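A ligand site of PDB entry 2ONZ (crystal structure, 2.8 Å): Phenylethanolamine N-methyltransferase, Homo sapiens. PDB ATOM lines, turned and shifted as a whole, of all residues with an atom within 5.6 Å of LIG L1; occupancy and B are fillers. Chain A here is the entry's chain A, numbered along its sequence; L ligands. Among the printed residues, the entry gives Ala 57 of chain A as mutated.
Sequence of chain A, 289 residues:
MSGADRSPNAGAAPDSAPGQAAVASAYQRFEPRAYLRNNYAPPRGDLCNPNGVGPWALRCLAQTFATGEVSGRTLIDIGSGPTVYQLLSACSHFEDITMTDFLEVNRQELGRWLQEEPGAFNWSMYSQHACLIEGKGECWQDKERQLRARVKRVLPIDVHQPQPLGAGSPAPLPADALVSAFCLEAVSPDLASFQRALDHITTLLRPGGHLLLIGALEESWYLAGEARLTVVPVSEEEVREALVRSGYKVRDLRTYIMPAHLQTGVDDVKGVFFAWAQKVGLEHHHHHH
An oxygen (O1) of LG2 L2 is in hydrogen-bond range of the side-chain hydroxyl of Tyr 40. O2 of LG2 L2 lies within hydrogen-bond range of OH of Tyr 85 (2.8 Å). The side-chain carboxylate of Glu 219 lies within salt-bridge range of a nitrogen (N2) of LIG L1 (2.8 Å). N2 of LIG L1 is in salt-bridge range of OD2 of Asp 267, 3.7 Å away. A nitrogen (N1) of LIG L1 lies within hydrogen-bond range of the backbone carbonyl oxygen (O) of Asn 39, 2.9 Å away. The side-chain hydroxyl (OH) of Tyr 35 sits at hydrogen-bond distance from an oxygen (O1) of LG2 L2 (2.6 Å).
The backbone NH (N) of Val 269 is in hydrogen-bond range of the side-chain carboxylate (OD1) of Asp 267 (3.1 Å). NH1 of Arg 44 lies within salt-bridge range of OD2 of Asp 267 (2.8 Å). The side-chain hydroxyl (OH) of Tyr 40 lies within hydrogen-bond range of the side-chain hydroxyl (OH) of Tyr 85. The guanidinium group (NH1) of Arg 44 lies within hydrogen-bond range of the side-chain amide oxygen (OD1) of Asn 39. The backbone carbonyl oxygen of Tyr 40 is in hydrogen-bond range of the side-chain hydroxyl of Tyr 126, at 2.7 Å. ND2 of Asn 39 sits at hydrogen-bond distance from O of Tyr 35, 2.9 Å away.
Residues that only touch LIG L1: Arg 44 (3.1 Å), Tyr 35 (3.2 Å), Val 53 (3.3 Å), Gly 54 (3.4 Å), Phe 182 (3.4 Å), Tyr 85 (3.5 Å), Met 258 (3.5 Å), Tyr 40 (3.6 Å), Tyr 222 (3.6 Å), Tyr 126 (3.7 Å), Val 272 (3.8 Å), Leu 58 (3.8 Å) and Ala 57 (3.99 Å). Hydrophobic or aromatic side chains within 4 Å of LIG L1: Tyr 35, Tyr 40, Val 53, Ala 57, Leu 58, Tyr 85, Tyr 126, Phe 182, Tyr 222, Met 258 and Val 272. 16 residues have an atom within 4 Å of LIG L1: Tyr 35, Asn 39, Tyr 40, Arg 44, Val 53, Gly 54, Ala 57, Leu 58, Tyr 85, Tyr 126, Phe 182, Glu 219, Tyr 222, Met 258, Asp 267 and Val 272. The nearest printed residue that does not touch LIG L1 is Val 269 (4.5 Å).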
ATOM      1  N   TYR A  35      12.132   3.963 -25.342  1.00  0.00           N
ATOM      2  CA  TYR A  35      12.428   5.128 -24.536  1.00  0.00           C
ATOM      3  C   TYR A  35      12.480   6.413 -25.383  1.00  0.00           C
ATOM      4  O   TYR A  35      11.913   7.447 -25.007  1.00  0.00           O
ATOM      5  CB  TYR A  35      13.775   4.930 -23.854  1.00  0.00           C
ATOM      6  CG  TYR A  35      14.227   6.129 -23.074  1.00  0.00           C
ATOM      7  CD1 TYR A  35      13.785   6.344 -21.767  1.00  0.00           C
ATOM      8  CD2 TYR A  35      15.107   7.060 -23.626  1.00  0.00           C
ATOM      9  CE1 TYR A  35      14.195   7.436 -21.049  1.00  0.00           C
ATOM     10  CE2 TYR A  35      15.534   8.166 -22.903  1.00  0.00           C
ATOM     11  CZ  TYR A  35      15.073   8.339 -21.615  1.00  0.00           C
ATOM     12  OH  TYR A  35      15.496   9.415 -20.873  1.00  0.00           O
ATOM     13  N   ASN A  39       9.814   9.663 -25.286  1.00  0.00           N
ATOM     14  CA  ASN A  39      10.251  10.981 -24.828  1.00  0.00           C
ATOM     15  C   ASN A  39      10.793  11.965 -25.830  1.00  0.00           C
ATOM     16  O   ASN A  39      10.809  13.170 -25.556  1.00  0.00           O
ATOM     17  CB  ASN A  39      11.291  10.792 -23.726  1.00  0.00           C
ATOM     18  CG  ASN A  39      10.782   9.912 -22.618  1.00  0.00           C
ATOM     19  OD1 ASN A  39       9.880  10.295 -21.889  1.00  0.00           O
ATOM     20  ND2 ASN A  39      11.363   8.725 -22.496  1.00  0.00           N
ATOM     21  N   TYR A  40      11.266  11.496 -26.978  1.00  0.00           N
ATOM     22  CA  TYR A  40      11.827  12.410 -27.951  1.00  0.00           C
ATOM     23  C   TYR A  40      11.136  12.417 -29.297  1.00  0.00           C
ATOM     24  O   TYR A  40      11.570  13.110 -30.232  1.00  0.00           O
ATOM     25  CB  TYR A  40      13.320  12.151 -28.093  1.00  0.00           C
ATOM     26  CG  TYR A  40      14.037  12.368 -26.793  1.00  0.00           C
ATOM     27  CD1 TYR A  40      14.264  11.312 -25.920  1.00  0.00           C
ATOM     28  CD2 TYR A  40      14.459  13.644 -26.411  1.00  0.00           C
ATOM     29  CE1 TYR A  40      14.891  11.520 -24.691  1.00  0.00           C
ATOM     30  CE2 TYR A  40      15.076  13.860 -25.189  1.00  0.00           C
ATOM     31  CZ  TYR A  40      15.293  12.797 -24.341  1.00  0.00           C
ATOM     32  OH  TYR A  40      15.892  12.999 -23.124  1.00  0.00           O
ATOM     33  N   ARG A  44       6.183  15.032 -27.215  1.00  0.00           N
ATOM     34  CA  ARG A  44       7.196  15.562 -26.325  1.00  0.00           C
ATOM     35  C   ARG A  44       8.481  15.933 -27.030  1.00  0.00           C
ATOM     36  O   ARG A  44       9.412  16.436 -26.416  1.00  0.00           O
ATOM     37  CB  ARG A  44       7.525  14.552 -25.237  1.00  0.00           C
ATOM     38  CG  ARG A  44       6.504  14.504 -24.149  1.00  0.00           C
ATOM     39  CD  ARG A  44       6.905  13.455 -23.182  1.00  0.00           C
ATOM     40  NE  ARG A  44       5.994  13.412 -22.061  1.00  0.00           N
ATOM     41  CZ  ARG A  44       6.258  12.775 -20.940  1.00  0.00           C
ATOM     42  NH1 ARG A  44       7.415  12.142 -20.812  1.00  0.00           N
ATOM     43  NH2 ARG A  44       5.391  12.782 -19.946  1.00  0.00           N
ATOM     44  N   GLY A  45       8.521  15.688 -28.333  1.00  0.00           N
ATOM     45  CA  GLY A  45       9.700  15.994 -29.103  1.00  0.00           C
ATOM     46  C   GLY A  45       9.485  17.086 -30.118  1.00  0.00           C
ATOM     47  O   GLY A  45      10.461  17.583 -30.682  1.00  0.00           O
ATOM     48  N   LEU A  47       9.493  20.358 -31.764  1.00  0.00           N
ATOM     49  CA  LEU A  47      10.252  21.537 -31.433  1.00  0.00           C
ATOM     50  C   LEU A  47       9.664  22.787 -32.077  1.00  0.00           C
ATOM     51  O   LEU A  47      10.106  23.892 -31.810  1.00  0.00           O
ATOM     52  CB  LEU A  47      11.703  21.327 -31.873  1.00  0.00           C
ATOM     53  CG  LEU A  47      12.287  20.038 -31.271  1.00  0.00           C
ATOM     54  CD1 LEU A  47      13.668  19.774 -31.809  1.00  0.00           C
ATOM     55  CD2 LEU A  47      12.316  20.170 -29.764  1.00  0.00           C
ATOM     56  N   VAL A  53       8.636  21.333 -23.987  1.00  0.00           N
ATOM     57  CA  VAL A  53       9.759  21.060 -23.099  1.00  0.00           C
ATOM     58  C   VAL A  53      11.053  21.024 -23.915  1.00  0.00           C
ATOM     59  O   VAL A  53      12.097  21.493 -23.470  1.00  0.00           O
ATOM     60  CB  VAL A  53       9.559  19.704 -22.336  1.00  0.00           C
ATOM     61  CG1 VAL A  53       9.526  18.533 -23.317  1.00  0.00           C
ATOM     62  CG2 VAL A  53      10.671  19.503 -21.307  1.00  0.00           C
ATOM     63  N   GLY A  54      10.978  20.482 -25.131  1.00  0.00           N
ATOM     64  CA  GLY A  54      12.153  20.406 -25.974  1.00  0.00           C
ATOM     65  C   GLY A  54      12.772  21.773 -26.197  1.00  0.00           C
ATOM     66  O   GLY A  54      13.942  21.995 -25.863  1.00  0.00           O
ATOM     67  N   PRO A  55      12.021  22.716 -26.763  1.00  0.00           N
ATOM     68  CA  PRO A  55      12.594  24.046 -26.987  1.00  0.00           C
ATOM     69  C   PRO A  55      13.217  24.587 -25.698  1.00  0.00           C
ATOM     70  O   PRO A  55      14.368  25.009 -25.678  1.00  0.00           O
ATOM     71  CB  PRO A  55      11.394  24.834 -27.460  1.00  0.00           C
ATOM     72  CG  PRO A  55      10.657  23.809 -28.282  1.00  0.00           C
ATOM     73  CD  PRO A  55      10.682  22.607 -27.379  1.00  0.00           C
ATOM     74  N   ALA A  57      14.381  23.089 -22.887  1.00  0.00           N
ATOM     75  CA  ALA A  57      15.619  22.398 -22.504  1.00  0.00           C
ATOM     76  C   ALA A  57      16.831  22.755 -23.366  1.00  0.00           C
ATOM     77  O   ALA A  57      17.904  23.045 -22.848  1.00  0.00           O
ATOM     78  CB  ALA A  57      15.397  20.900 -22.529  1.00  0.00           C
ATOM     79  N   LEU A  58      16.656  22.716 -24.692  1.00  0.00           N
ATOM     80  CA  LEU A  58      17.767  23.065 -25.590  1.00  0.00           C
ATOM     81  C   LEU A  58      18.196  24.520 -25.343  1.00  0.00           C
ATOM     82  O   LEU A  58      19.368  24.886 -25.480  1.00  0.00           O
ATOM     83  CB  LEU A  58      17.343  22.914 -27.043  1.00  0.00           C
ATOM     84  CG  LEU A  58      17.196  21.498 -27.556  1.00  0.00           C
ATOM     85  CD1 LEU A  58      16.780  21.549 -29.018  1.00  0.00           C
ATOM     86  CD2 LEU A  58      18.509  20.743 -27.399  1.00  0.00           C
ATOM     87  N   TYR A  85      21.116  14.984 -27.773  1.00  0.00           N
ATOM     88  CA  TYR A  85      20.716  16.381 -27.707  1.00  0.00           C
ATOM     89  C   TYR A  85      21.457  17.115 -26.595  1.00  0.00           C
ATOM     90  O   TYR A  85      21.947  18.233 -26.793  1.00  0.00           O
ATOM     91  CB  TYR A  85      19.202  16.488 -27.471  1.00  0.00           C
ATOM     92  CG  TYR A  85      18.772  16.118 -26.074  1.00  0.00           C
ATOM     93  CD1 TYR A  85      18.597  17.091 -25.100  1.00  0.00           C
ATOM     94  CD2 TYR A  85      18.561  14.796 -25.712  1.00  0.00           C
ATOM     95  CE1 TYR A  85      18.213  16.762 -23.812  1.00  0.00           C
ATOM     96  CE2 TYR A  85      18.178  14.448 -24.434  1.00  0.00           C
ATOM     97  CZ  TYR A  85      18.003  15.443 -23.484  1.00  0.00           C
ATOM     98  OH  TYR A  85      17.614  15.110 -22.208  1.00  0.00           O
ATOM     99  N   TYR A 126      16.648  18.205 -33.832  1.00  0.00           N
ATOM    100  CA  TYR A 126      17.235  18.794 -32.638  1.00  0.00           C
ATOM    101  C   TYR A 126      18.478  19.605 -32.984  1.00  0.00           C
ATOM    102  O   TYR A 126      18.626  20.732 -32.518  1.00  0.00           O
ATOM    103  CB  TYR A 126      17.586  17.708 -31.616  1.00  0.00           C
ATOM    104  CG  TYR A 126      16.386  17.045 -30.960  1.00  0.00           C
ATOM    105  CD1 TYR A 126      15.551  16.206 -31.695  1.00  0.00           C
ATOM    106  CD2 TYR A 126      16.085  17.247 -29.611  1.00  0.00           C
ATOM    107  CE1 TYR A 126      14.450  15.579 -31.113  1.00  0.00           C
ATOM    108  CE2 TYR A 126      14.989  16.624 -29.017  1.00  0.00           C
ATOM    109  CZ  TYR A 126      14.168  15.793 -29.783  1.00  0.00           C
ATOM    110  OH  TYR A 126      13.082  15.137 -29.230  1.00  0.00           O
ATOM    111  N   PHE A 182      18.518  13.350 -16.763  1.00  0.00           N
ATOM    112  CA  PHE A 182      17.618  12.265 -16.401  1.00  0.00           C
ATOM    113  C   PHE A 182      18.294  10.968 -15.953  1.00  0.00           C
ATOM    114  O   PHE A 182      17.796   9.874 -16.240  1.00  0.00           O
ATOM    115  CB  PHE A 182      16.667  11.958 -17.581  1.00  0.00           C
ATOM    116  CG  PHE A 182      15.861  13.145 -18.047  1.00  0.00           C
ATOM    117  CD1 PHE A 182      16.160  13.771 -19.248  1.00  0.00           C
ATOM    118  CD2 PHE A 182      14.803  13.620 -17.283  1.00  0.00           C
ATOM    119  CE1 PHE A 182      15.398  14.866 -19.689  1.00  0.00           C
ATOM    120  CE2 PHE A 182      14.037  14.706 -17.727  1.00  0.00           C
ATOM    121  CZ  PHE A 182      14.336  15.333 -18.928  1.00  0.00           C
ATOM    122  N   GLU A 185      18.284  10.698 -10.721  1.00  0.00           N
ATOM    123  CA  GLU A 185      16.992  10.400 -10.113  1.00  0.00           C
ATOM    124  C   GLU A 185      16.351   9.156 -10.710  1.00  0.00           C
ATOM    125  O   GLU A 185      15.479   8.563 -10.096  1.00  0.00           O
ATOM    126  CB  GLU A 185      16.026  11.607 -10.229  1.00  0.00           C
ATOM    127  CG  GLU A 185      15.301  11.808 -11.572  1.00  0.00           C
ATOM    128  CD  GLU A 185      16.123  12.533 -12.633  1.00  0.00           C
ATOM    129  OE1 GLU A 185      17.197  13.062 -12.296  1.00  0.00           O
ATOM    130  OE2 GLU A 185      15.667  12.585 -13.794  1.00  0.00           O
ATOM    131  N   ALA A 186      16.778   8.750 -11.898  1.00  0.00           N
ATOM    132  CA  ALA A 186      16.184   7.583 -12.529  1.00  0.00           C
ATOM    133  C   ALA A 186      16.869   6.303 -12.072  1.00  0.00           C
ATOM    134  O   ALA A 186      16.436   5.213 -12.435  1.00  0.00           O
ATOM    135  CB  ALA A 186      16.269   7.716 -14.049  1.00  0.00           C
ATOM    136  N   ALA A 216      14.033  14.904 -14.093  1.00  0.00           N
ATOM    137  CA  ALA A 216      12.603  14.915 -13.839  1.00  0.00           C
ATOM    138  C   ALA A 216      12.221  15.393 -12.437  1.00  0.00           C
ATOM    139  O   ALA A 216      12.823  15.006 -11.447  1.00  0.00           O
ATOM    140  CB  ALA A 216      12.044  13.511 -14.064  1.00  0.00           C
ATOM    141  N   GLU A 219       8.975  12.822 -10.311  1.00  0.00           N
ATOM    142  CA  GLU A 219       8.635  11.618 -11.040  1.00  0.00           C
ATOM    143  C   GLU A 219       8.961  10.370 -10.212  1.00  0.00           C
ATOM    144  O   GLU A 219      10.054  10.268  -9.640  1.00  0.00           O
ATOM    145  CB  GLU A 219       9.375  11.543 -12.381  1.00  0.00           C
ATOM    146  CG  GLU A 219       9.199  10.193 -13.062  1.00  0.00           C
ATOM    147  CD  GLU A 219      10.053  10.024 -14.286  1.00  0.00           C
ATOM    148  OE1 GLU A 219       9.549  10.346 -15.390  1.00  0.00           O
ATOM    149  OE2 GLU A 219      11.213   9.583 -14.137  1.00  0.00           O
ATOM    150  N   TYR A 222       8.649   5.624 -14.835  1.00  0.00           N
ATOM    151  CA  TYR A 222       8.549   5.908 -16.263  1.00  0.00           C
ATOM    152  C   TYR A 222       8.800   4.615 -17.005  1.00  0.00           C
ATOM    153  O   TYR A 222       9.584   3.781 -16.556  1.00  0.00           O
ATOM    154  CB  TYR A 222       9.549   7.002 -16.667  1.00  0.00           C
ATOM    155  CG  TYR A 222      10.989   6.554 -16.708  1.00  0.00           C
ATOM    156  CD1 TYR A 222      11.535   6.023 -17.875  1.00  0.00           C
ATOM    157  CD2 TYR A 222      11.802   6.648 -15.575  1.00  0.00           C
ATOM    158  CE1 TYR A 222      12.853   5.612 -17.924  1.00  0.00           C
ATOM    159  CE2 TYR A 222      13.124   6.241 -15.612  1.00  0.00           C
ATOM    160  CZ  TYR A 222      13.644   5.721 -16.804  1.00  0.00           C
ATOM    161  OH  TYR A 222      14.961   5.315 -16.863  1.00  0.00           O
ATOM    162  N   MET A 258       5.394  20.439 -16.616  1.00  0.00           N
ATOM    163  CA  MET A 258       4.868  19.671 -17.741  1.00  0.00           C
ATOM    164  C   MET A 258       3.413  20.054 -18.039  1.00  0.00           C
ATOM    165  O   MET A 258       2.587  20.113 -17.148  1.00  0.00           O
ATOM    166  CB  MET A 258       4.988  18.168 -17.427  1.00  0.00           C
ATOM    167  CG  MET A 258       5.169  17.292 -18.668  1.00  0.00           C
ATOM    168  SD  MET A 258       6.627  17.745 -19.649  1.00  0.00           S
ATOM    169  CE  MET A 258       7.869  16.643 -19.027  1.00  0.00           C
ATOM    170  N   ASP A 267       4.753   8.005 -18.183  1.00  0.00           N
ATOM    171  CA  ASP A 267       5.310   8.254 -16.867  1.00  0.00           C
ATOM    172  C   ASP A 267       4.379   9.119 -16.065  1.00  0.00           C
ATOM    173  O   ASP A 267       3.242   9.370 -16.475  1.00  0.00           O
ATOM    174  CB  ASP A 267       6.687   8.914 -16.969  1.00  0.00           C
ATOM    175  CG  ASP A 267       6.694  10.209 -17.794  1.00  0.00           C
ATOM    176  OD1 ASP A 267       5.894  11.138 -17.498  1.00  0.00           O
ATOM    177  OD2 ASP A 267       7.513  10.309 -18.737  1.00  0.00           O
ATOM    178  N   VAL A 269       5.774  12.101 -14.528  1.00  0.00           N
ATOM    179  CA  VAL A 269       6.574  13.313 -14.310  1.00  0.00           C
ATOM    180  C   VAL A 269       5.665  14.554 -14.166  1.00  0.00           C
ATOM    181  O   VAL A 269       4.615  14.635 -14.789  1.00  0.00           O
ATOM    182  CB  VAL A 269       7.568  13.538 -15.495  1.00  0.00           C
ATOM    183  CG1 VAL A 269       6.818  14.037 -16.735  1.00  0.00           C
ATOM    184  CG2 VAL A 269       8.665  14.517 -15.097  1.00  0.00           C
ATOM    185  N   VAL A 272      10.283  19.334 -15.336  1.00  0.00           N
ATOM    186  CA  VAL A 272      11.680  19.017 -15.620  1.00  0.00           C
ATOM    187  C   VAL A 272      12.507  20.165 -15.031  1.00  0.00           C
ATOM    188  O   VAL A 272      12.046  21.301 -14.956  1.00  0.00           O
ATOM    189  CB  VAL A 272      11.914  18.886 -17.162  1.00  0.00           C
ATOM    190  CG1 VAL A 272      13.400  18.827 -17.471  1.00  0.00           C
ATOM    191  CG2 VAL A 272      11.226  17.633 -17.689  1.00  0.00           C
HETATM  192  C1  LIG L   1      13.320  10.397 -18.673  1.00  0.00           C
HETATM  193  C2  LIG L   1      12.375  15.903 -23.910  1.00  0.00           C
HETATM  194  C3  LIG L   1      14.287  17.590 -25.047  1.00  0.00           C
HETATM  195  C4  LIG L   1      14.435  17.159 -23.736  1.00  0.00           C
HETATM  196  C5  LIG L   1      13.184  17.176 -25.785  1.00  0.00           C
HETATM  197  C6  LIG L   1      13.479  16.313 -23.163  1.00  0.00           C
HETATM  198  C7  LIG L   1      12.222  16.346 -25.215  1.00  0.00           C
HETATM  199  C8  LIG L   1      13.405  12.131 -20.507  1.00  0.00           C
HETATM  200  C9  LIG L   1      11.452  12.083 -19.100  1.00  0.00           C
HETATM  201  C10 LIG L   1      12.500  10.018 -17.433  1.00  0.00           C
HETATM  202  C11 LIG L   1      10.643  11.457 -17.956  1.00  0.00           C
HETATM  203 CL1  LIG L   1      15.494  18.584 -25.781  1.00  0.00          CL
HETATM  204  N1  LIG L   1      11.394  14.953 -23.343  1.00  0.00           N
HETATM  205  S1  LIG L   1      10.932  15.038 -21.784  1.00  0.00           S
HETATM  206  O1  LIG L   1      11.383  16.264 -21.217  1.00  0.00           O
HETATM  207  O2  LIG L   1       9.439  14.960 -21.715  1.00  0.00           O
HETATM  208  C12 LIG L   1      11.621  13.695 -20.884  1.00  0.00           C
HETATM  209  C13 LIG L   1      10.919  13.143 -19.828  1.00  0.00           C
HETATM  210  C14 LIG L   1      12.873  13.186 -21.226  1.00  0.00           C
HETATM  211  C15 LIG L   1      12.705  11.570 -19.433  1.00  0.00           C
HETATM  212  N2  LIG L   1      11.072  10.064 -17.751  1.00  0.00           N
HETATM  213  N1  LG2 L   2      20.467  10.840 -20.557  1.00  0.00           N
HETATM  214  C1  LG2 L   2      19.357  10.348 -21.380  1.00  0.00           C
HETATM  215  C2  LG2 L   2      18.760   9.056 -20.770  1.00  0.00           C
HETATM  216  C3  LG2 L   2      18.337   9.133 -19.288  1.00  0.00           C
HETATM  217  S1  LG2 L   2      17.473   7.644 -18.733  1.00  0.00           S
HETATM  218  C4  LG2 L   2      18.280  11.415 -21.600  1.00  0.00           C
HETATM  219  O1  LG2 L   2      17.138  11.064 -21.993  1.00  0.00           O
HETATM  220  O2  LG2 L   2      18.597  12.616 -21.414  1.00  0.00           O
HETATM  221  C5  LG2 L   2      18.563   6.985 -17.463  1.00  0.00           C
HETATM  222  C6  LG2 L   2      19.817   6.346 -18.020  1.00  0.00           C
HETATM  223  O3  LG2 L   2      20.734   5.978 -16.949  1.00  0.00           O
HETATM  224  C7  LG2 L   2      19.651   5.127 -18.917  1.00  0.00           C
HETATM  225  O4  LG2 L   2      20.378   5.297 -20.129  1.00  0.00           O
HETATM  226  C8  LG2 L   2      20.220   3.993 -18.062  1.00  0.00           C
HETATM  227  O5  LG2 L   2      20.797   2.979 -18.860  1.00  0.00           O
HETATM  228  C9  LG2 L   2      21.282   4.714 -17.249  1.00  0.00           C
HETATM  229  N2  LG2 L   2      21.678   4.081 -15.985  1.00  0.00           N
HETATM  230  C10 LG2 L   2      21.060   3.007 -15.282  1.00  0.00           C
HETATM  231  N3  LG2 L   2      21.700   2.670 -14.181  1.00  0.00           N
HETATM  232  C11 LG2 L   2      22.770   3.549 -14.161  1.00  0.00           C
HETATM  233  C12 LG2 L   2      23.814   3.659 -13.221  1.00  0.00           C
HETATM  234  N4  LG2 L   2      23.919   2.877 -12.144  1.00  0.00           N
HETATM  235  N5  LG2 L   2      24.754   4.618 -13.426  1.00  0.00           N
HETATM  236  C13 LG2 L   2      24.641   5.405 -14.534  1.00  0.00           C
HETATM  237  N6  LG2 L   2      23.690   5.388 -15.483  1.00  0.00           N
HETATM  238  C14 LG2 L   2      22.781   4.421 -15.241  1.00  0.00           C
